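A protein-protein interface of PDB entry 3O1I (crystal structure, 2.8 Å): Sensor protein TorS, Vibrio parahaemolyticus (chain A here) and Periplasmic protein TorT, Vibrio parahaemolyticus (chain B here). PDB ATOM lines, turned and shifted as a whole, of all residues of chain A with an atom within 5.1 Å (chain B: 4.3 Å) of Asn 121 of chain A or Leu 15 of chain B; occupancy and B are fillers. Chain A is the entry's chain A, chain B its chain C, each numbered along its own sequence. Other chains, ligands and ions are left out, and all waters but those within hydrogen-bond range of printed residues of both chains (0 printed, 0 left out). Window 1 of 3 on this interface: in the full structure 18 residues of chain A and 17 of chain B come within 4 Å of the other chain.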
ATOM      1  N   THR A 117       2.272  18.202   2.160  1.00  0.00           N
ATOM      2  CA  THR A 117       0.921  18.488   2.630  1.00  0.00           C
ATOM      3  C   THR A 117       0.935  19.022   4.069  1.00  0.00           C
ATOM      4  O   THR A 117       0.173  19.931   4.399  1.00  0.00           O
ATOM      5  CB  THR A 117      -0.008  17.235   2.575  1.00  0.00           C
ATOM      6  OG1 THR A 117       0.469  16.251   3.492  1.00  0.00           O
ATOM      7  CG2 THR A 117      -0.036  16.638   1.174  1.00  0.00           C
ATOM      8  N   GLN A 118       1.795  18.482   4.923  1.00  0.00           N
ATOM      9  CA  GLN A 118       1.839  18.962   6.291  1.00  0.00           C
ATOM     10  C   GLN A 118       2.302  20.408   6.330  1.00  0.00           C
ATOM     11  O   GLN A 118       1.830  21.216   7.125  1.00  0.00           O
ATOM     12  CB  GLN A 118       2.761  18.091   7.126  1.00  0.00           C
ATOM     13  CG  GLN A 118       2.270  16.669   7.248  1.00  0.00           C
ATOM     14  CD  GLN A 118       3.113  15.848   8.204  1.00  0.00           C
ATOM     15  OE1 GLN A 118       3.079  16.058   9.417  1.00  0.00           O
ATOM     16  NE2 GLN A 118       3.884  14.907   7.657  1.00  0.00           N
ATOM     17  N   VAL A 119       3.237  20.725   5.454  1.00  0.00           N
ATOM     18  CA  VAL A 119       3.773  22.068   5.367  1.00  0.00           C
ATOM     19  C   VAL A 119       2.645  23.056   5.049  1.00  0.00           C
ATOM     20  O   VAL A 119       2.480  24.081   5.720  1.00  0.00           O
ATOM     21  CB  VAL A 119       4.895  22.118   4.272  1.00  0.00           C
ATOM     22  CG1 VAL A 119       5.067  23.528   3.719  1.00  0.00           C
ATOM     23  CG2 VAL A 119       6.218  21.591   4.867  1.00  0.00           C
ATOM     24  N   GLN A 120       1.845  22.731   4.045  1.00  0.00           N
ATOM     25  CA  GLN A 120       0.762  23.607   3.638  1.00  0.00           C
ATOM     26  C   GLN A 120      -0.422  23.677   4.612  1.00  0.00           C
ATOM     27  O   GLN A 120      -1.154  24.682   4.651  1.00  0.00           O
ATOM     28  CB  GLN A 120       0.320  23.215   2.240  1.00  0.00           C
ATOM     29  CG  GLN A 120       1.509  23.209   1.322  1.00  0.00           C
ATOM     30  CD  GLN A 120       1.136  23.083  -0.121  1.00  0.00           C
ATOM     31  OE1 GLN A 120       0.483  22.121  -0.526  1.00  0.00           O
ATOM     32  NE2 GLN A 120       1.559  24.058  -0.924  1.00  0.00           N
ATOM     33  N   ASN A 121      -0.608  22.619   5.399  1.00  0.00           N
ATOM     34  CA  ASN A 121      -1.663  22.619   6.396  1.00  0.00           C
ATOM     35  C   ASN A 121      -1.155  23.563   7.479  1.00  0.00           C
ATOM     36  O   ASN A 121      -1.850  24.497   7.872  1.00  0.00           O
ATOM     37  CB  ASN A 121      -1.869  21.223   6.992  1.00  0.00           C
ATOM     38  CG  ASN A 121      -2.511  20.256   6.015  1.00  0.00           C
ATOM     39  OD1 ASN A 121      -3.011  20.657   4.951  1.00  0.00           O
ATOM     40  ND2 ASN A 121      -2.516  18.969   6.374  1.00  0.00           N
ATOM     41  N   THR A 122       0.074  23.325   7.930  1.00  0.00           N
ATOM     42  CA  THR A 122       0.689  24.139   8.974  1.00  0.00           C
ATOM     43  C   THR A 122       0.687  25.628   8.662  1.00  0.00           C
ATOM     44  O   THR A 122       0.697  26.450   9.577  1.00  0.00           O
ATOM     45  CB  THR A 122       2.151  23.699   9.278  1.00  0.00           C
ATOM     46  OG1 THR A 122       2.147  22.438   9.968  1.00  0.00           O
ATOM     47  CG2 THR A 122       2.847  24.726  10.157  1.00  0.00           C
ATOM     48  N   SER A 123       0.673  25.989   7.385  1.00  0.00           N
ATOM     49  CA  SER A 123       0.661  27.404   7.059  1.00  0.00           C
ATOM     50  C   SER A 123      -0.784  27.910   7.144  1.00  0.00           C
ATOM     51  O   SER A 123      -1.046  28.968   7.722  1.00  0.00           O
ATOM     52  CB  SER A 123       1.259  27.653   5.665  1.00  0.00           C
ATOM     53  OG  SER A 123       0.374  27.274   4.629  1.00  0.00           O
ATOM     54  N   THR A 124      -1.719  27.149   6.578  1.00  0.00           N
ATOM     55  CA  THR A 124      -3.128  27.517   6.611  1.00  0.00           C
ATOM     56  C   THR A 124      -3.585  27.753   8.053  1.00  0.00           C
ATOM     57  O   THR A 124      -4.235  28.742   8.361  1.00  0.00           O
ATOM     58  CB  THR A 124      -4.002  26.407   6.008  1.00  0.00           C
ATOM     59  OG1 THR A 124      -3.764  26.325   4.599  1.00  0.00           O
ATOM     60  CG2 THR A 124      -5.481  26.692   6.263  1.00  0.00           C
ATOM     61  N   ILE A 125      -3.229  26.828   8.932  1.00  0.00           N
ATOM     62  CA  ILE A 125      -3.596  26.908  10.336  1.00  0.00           C
ATOM     63  C   ILE A 125      -2.927  28.095  11.028  1.00  0.00           C
ATOM     64  O   ILE A 125      -3.319  28.500  12.126  1.00  0.00           O
ATOM     65  CB  ILE A 125      -3.218  25.595  11.038  1.00  0.00           C
ATOM     66  CG1 ILE A 125      -3.975  24.445  10.367  1.00  0.00           C
ATOM     67  CG2 ILE A 125      -3.531  25.666  12.524  1.00  0.00           C
ATOM     68  CD1 ILE A 125      -3.494  23.062  10.780  1.00  0.00           C
ATOM     69  N   ALA A 126      -1.912  28.655  10.384  1.00  0.00           N
ATOM     70  CA  ALA A 126      -1.217  29.801  10.950  1.00  0.00           C
ATOM     71  C   ALA A 126      -2.096  31.013  10.683  1.00  0.00           C
ATOM     72  O   ALA A 126      -2.317  31.838  11.565  1.00  0.00           O
ATOM     73  CB  ALA A 126       0.135  29.967  10.295  1.00  0.00           C
ATOM     74  N   ARG A 215      -0.088  11.137  12.389  1.00  0.00           N
ATOM     75  CA  ARG A 215       0.611  11.239  11.125  1.00  0.00           C
ATOM     76  C   ARG A 215       2.072  10.871  11.323  1.00  0.00           C
ATOM     77  O   ARG A 215       2.764  10.524  10.368  1.00  0.00           O
ATOM     78  CB  ARG A 215       0.472  12.640  10.542  1.00  0.00           C
ATOM     79  CG  ARG A 215       0.100  12.592   9.081  1.00  0.00           C
ATOM     80  CD  ARG A 215      -0.417  13.902   8.574  1.00  0.00           C
ATOM     81  NE  ARG A 215      -1.284  13.666   7.431  1.00  0.00           N
ATOM     82  CZ  ARG A 215      -1.960  14.617   6.801  1.00  0.00           C
ATOM     83  NH1 ARG A 215      -1.865  15.882   7.207  1.00  0.00           N
ATOM     84  NH2 ARG A 215      -2.744  14.295   5.778  1.00  0.00           N
ATOM     85  N   TYR B  12     -10.210  11.665  -0.716  1.00  0.00           N
ATOM     86  CA  TYR B  12      -9.958  13.005  -1.243  1.00  0.00           C
ATOM     87  C   TYR B  12      -8.934  12.971  -2.372  1.00  0.00           C
ATOM     88  O   TYR B  12      -8.327  11.939  -2.649  1.00  0.00           O
ATOM     89  CB  TYR B  12      -9.386  13.908  -0.168  1.00  0.00           C
ATOM     90  CG  TYR B  12     -10.130  13.946   1.138  1.00  0.00           C
ATOM     91  CD1 TYR B  12     -11.434  13.454   1.255  1.00  0.00           C
ATOM     92  CD2 TYR B  12      -9.550  14.554   2.254  1.00  0.00           C
ATOM     93  CE1 TYR B  12     -12.143  13.582   2.455  1.00  0.00           C
ATOM     94  CE2 TYR B  12     -10.244  14.682   3.445  1.00  0.00           C
ATOM     95  CZ  TYR B  12     -11.539  14.201   3.536  1.00  0.00           C
ATOM     96  OH  TYR B  12     -12.215  14.388   4.707  1.00  0.00           O
ATOM     97  N   HIS B  14      -6.540  15.167  -2.319  1.00  0.00           N
ATOM     98  CA  HIS B  14      -5.419  15.659  -1.515  1.00  0.00           C
ATOM     99  C   HIS B  14      -5.951  16.305  -0.236  1.00  0.00           C
ATOM    100  O   HIS B  14      -7.139  16.287   0.029  1.00  0.00           O
ATOM    101  CB  HIS B  14      -4.621  16.721  -2.262  1.00  0.00           C
ATOM    102  CG  HIS B  14      -5.360  18.008  -2.436  1.00  0.00           C
ATOM    103  ND1 HIS B  14      -5.982  18.358  -3.617  1.00  0.00           N
ATOM    104  CD2 HIS B  14      -5.611  19.012  -1.562  1.00  0.00           C
ATOM    105  CE1 HIS B  14      -6.587  19.523  -3.464  1.00  0.00           C
ATOM    106  NE2 HIS B  14      -6.378  19.939  -2.226  1.00  0.00           N
ATOM    107  N   LEU B  15      -5.059  16.877   0.556  1.00  0.00           N
ATOM    108  CA  LEU B  15      -5.458  17.563   1.767  1.00  0.00           C
ATOM    109  C   LEU B  15      -4.471  18.704   2.004  1.00  0.00           C
ATOM    110  O   LEU B  15      -3.818  18.789   3.047  1.00  0.00           O
ATOM    111  CB  LEU B  15      -5.483  16.614   2.968  1.00  0.00           C
ATOM    112  CG  LEU B  15      -6.359  17.088   4.150  1.00  0.00           C
ATOM    113  CD1 LEU B  15      -7.825  16.979   3.781  1.00  0.00           C
ATOM    114  CD2 LEU B  15      -6.102  16.243   5.387  1.00  0.00           C
ATOM    115  N   LYS B  16      -4.386  19.588   1.011  1.00  0.00           N
ATOM    116  CA  LYS B  16      -3.489  20.742   1.055  1.00  0.00           C
ATOM    117  C   LYS B  16      -4.226  22.092   1.129  1.00  0.00           C
ATOM    118  O   LYS B  16      -3.797  22.988   1.856  1.00  0.00           O
ATOM    119  CB  LYS B  16      -2.562  20.706  -0.165  1.00  0.00           C
ATOM    120  CG  LYS B  16      -1.705  19.454  -0.219  1.00  0.00           C
ATOM    121  CD  LYS B  16      -0.771  19.408  -1.428  1.00  0.00           C
ATOM    122  CE  LYS B  16      -1.530  19.209  -2.730  1.00  0.00           C
ATOM    123  NZ  LYS B  16      -0.612  18.953  -3.875  1.00  0.00           N
ATOM    124  N   ASP B  17      -5.317  22.225   0.366  1.00  0.00           N
ATOM    125  CA  ASP B  17      -6.166  23.427   0.345  1.00  0.00           C
ATOM    126  C   ASP B  17      -6.747  23.621   1.721  1.00  0.00           C
ATOM    127  O   ASP B  17      -6.708  22.715   2.548  1.00  0.00           O
ATOM    128  CB  ASP B  17      -7.399  23.244  -0.554  1.00  0.00           C
ATOM    129  CG  ASP B  17      -7.092  23.340  -2.017  1.00  0.00           C
ATOM    130  OD1 ASP B  17      -6.264  24.198  -2.389  1.00  0.00           O
ATOM    131  OD2 ASP B  17      -7.699  22.574  -2.804  1.00  0.00           O
ATOM    132  N   TRP B  20     -10.182  21.767   1.201  1.00  0.00           N
ATOM    133  CA  TRP B  20     -10.372  20.394   1.643  1.00  0.00           C
ATOM    134  C   TRP B  20     -10.037  20.224   3.104  1.00  0.00           C
ATOM    135  O   TRP B  20     -10.519  19.293   3.741  1.00  0.00           O
ATOM    136  CB  TRP B  20      -9.545  19.419   0.816  1.00  0.00           C
ATOM    137  CG  TRP B  20     -10.090  19.207  -0.558  1.00  0.00           C
ATOM    138  CD1 TRP B  20      -9.749  19.886  -1.691  1.00  0.00           C
ATOM    139  CD2 TRP B  20     -11.061  18.230  -0.952  1.00  0.00           C
ATOM    140  NE1 TRP B  20     -10.440  19.388  -2.776  1.00  0.00           N
ATOM    141  CE2 TRP B  20     -11.253  18.370  -2.351  1.00  0.00           C
ATOM    142  CE3 TRP B  20     -11.783  17.242  -0.263  1.00  0.00           C
ATOM    143  CZ2 TRP B  20     -12.138  17.561  -3.077  1.00  0.00           C
ATOM    144  CZ3 TRP B  20     -12.663  16.434  -0.986  1.00  0.00           C
ATOM    145  CH2 TRP B  20     -12.831  16.602  -2.385  1.00  0.00           C
ATOM    146  N   ASN B  24     -12.904  18.481   5.145  1.00  0.00           N
ATOM    147  CA  ASN B  24     -12.502  17.449   6.080  1.00  0.00           C
ATOM    148  C   ASN B  24     -13.309  17.578   7.351  1.00  0.00           C
ATOM    149  O   ASN B  24     -13.998  16.645   7.735  1.00  0.00           O
ATOM    150  CB  ASN B  24     -11.005  17.561   6.386  1.00  0.00           C
ATOM    151  CG  ASN B  24     -10.519  16.464   7.316  1.00  0.00           C
ATOM    152  OD1 ASN B  24     -10.191  16.716   8.479  1.00  0.00           O
ATOM    153  ND2 ASN B  24     -10.484  15.233   6.810  1.00  0.00           N
ATOM    154  N   GLU B  42      -6.116  10.327   1.473  1.00  0.00           N
ATOM    155  CA  GLU B  42      -5.934  11.396   0.505  1.00  0.00           C
ATOM    156  C   GLU B  42      -4.859  11.017  -0.503  1.00  0.00           C
ATOM    157  O   GLU B  42      -3.755  10.617  -0.129  1.00  0.00           O
ATOM    158  CB  GLU B  42      -5.587  12.702   1.233  1.00  0.00           C
ATOM    159  CG  GLU B  42      -4.240  12.713   1.923  1.00  0.00           C
ATOM    160  CD  GLU B  42      -3.179  13.406   1.094  1.00  0.00           C
ATOM    161  OE1 GLU B  42      -2.002  13.393   1.515  1.00  0.00           O
ATOM    162  OE2 GLU B  42      -3.520  13.974   0.027  1.00  0.00           O
ATOM    163  N   PRO B 301      -6.273  18.426  10.647  1.00  0.00           N
ATOM    164  CA  PRO B 301      -6.960  17.388   9.876  1.00  0.00           C
ATOM    165  C   PRO B 301      -6.796  16.036  10.569  1.00  0.00           C
ATOM    166  O   PRO B 301      -5.715  15.701  11.054  1.00  0.00           O
ATOM    167  CB  PRO B 301      -6.262  17.452   8.522  1.00  0.00           C
ATOM    168  CG  PRO B 301      -4.878  17.910   8.882  1.00  0.00           C
ATOM    169  CD  PRO B 301      -5.145  18.991   9.889  1.00  0.00           C
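The side-chain amide oxygen of Asn 121 of chain A lies close to the backbone carbonyl oxygen of Leu 15 of chain B, at 2.8 Å.
OG of Ser 123 of chain A is in hydrogen-bond range of O of Gln 120 of chain A (3.0 Å).
ND2 of Asn 121 of chain A sits close to NH1 of Arg 215 of chain A (3.3 Å).
The backbone NH of Leu 15 of chain B is in hydrogen-bond range of the side-chain carboxylate of Glu 42 of chain B (3.3 Å).
O of Thr 117 of chain A sits close to OD1 of Asn 121 of chain A (3.3 Å).
The backbone carbonyl oxygen of Gln 120 of chain A lies within hydrogen-bond range of the side-chain hydroxyl of Thr 124 of chain A, at 3.1 Å.
Among the printed residues, merely in contact across the chains: Gln 120 of chain A with Lys 16 of chain B, Thr 117 of chain A with Lys 16 of chain B, Asn 121 of chain A with Pro 301 of chain B, Thr 117 of chain A with Glu 42 of chain B, Arg 215 of chain A with Leu 15 of chain B, Asn 121 of chain A with Lys 16 of chain B and Arg 215 of chain A with Pro 301 of chain B.
Printed residues of chain B within 4 Å of Gln 120 of chain A: Lys 16.
Printed residues of chain B within 4 Å of Arg 215 of chain A: Leu 15 (3.9 Å) and Pro 301 (3.9996 Å).
Of chain A, only Asn 121 (2.8 Å) and Arg 215 (3.9 Å) come within 4 Å of Leu 15 of chain B.
Printed residues of chain A within 4 Å of Lys 16 of chain B: Thr 117, Gln 120 and Asn 121.
Trp 20 of chain B touches none of the printed residues of chain A.
Of the printed residues of chain A, Glu 42 of chain B touches Thr 117.
Printed residues of chain A within 4 Å of Pro 301 of chain B: Asn 121 and Arg 215.
The nearest printed residue of chain A that does not touch Pro 301 of chain B is Ile 125 of chain A (4.5 Å).
Of the 9 printed residues of chain B, 4 touch a printed residue of chain A.
Hydrophobic or aromatic side chains of chain B within 4 Å of the printed part of chain A: Leu 15 and Pro 301.
Of the 11 printed residues of chain A, 4 touch a printed residue of chain B.
Among the printed residues, no Asp or Glu carboxylate lies within 4 Å of a Lys or Arg side-chain nitrogen of the other chain.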
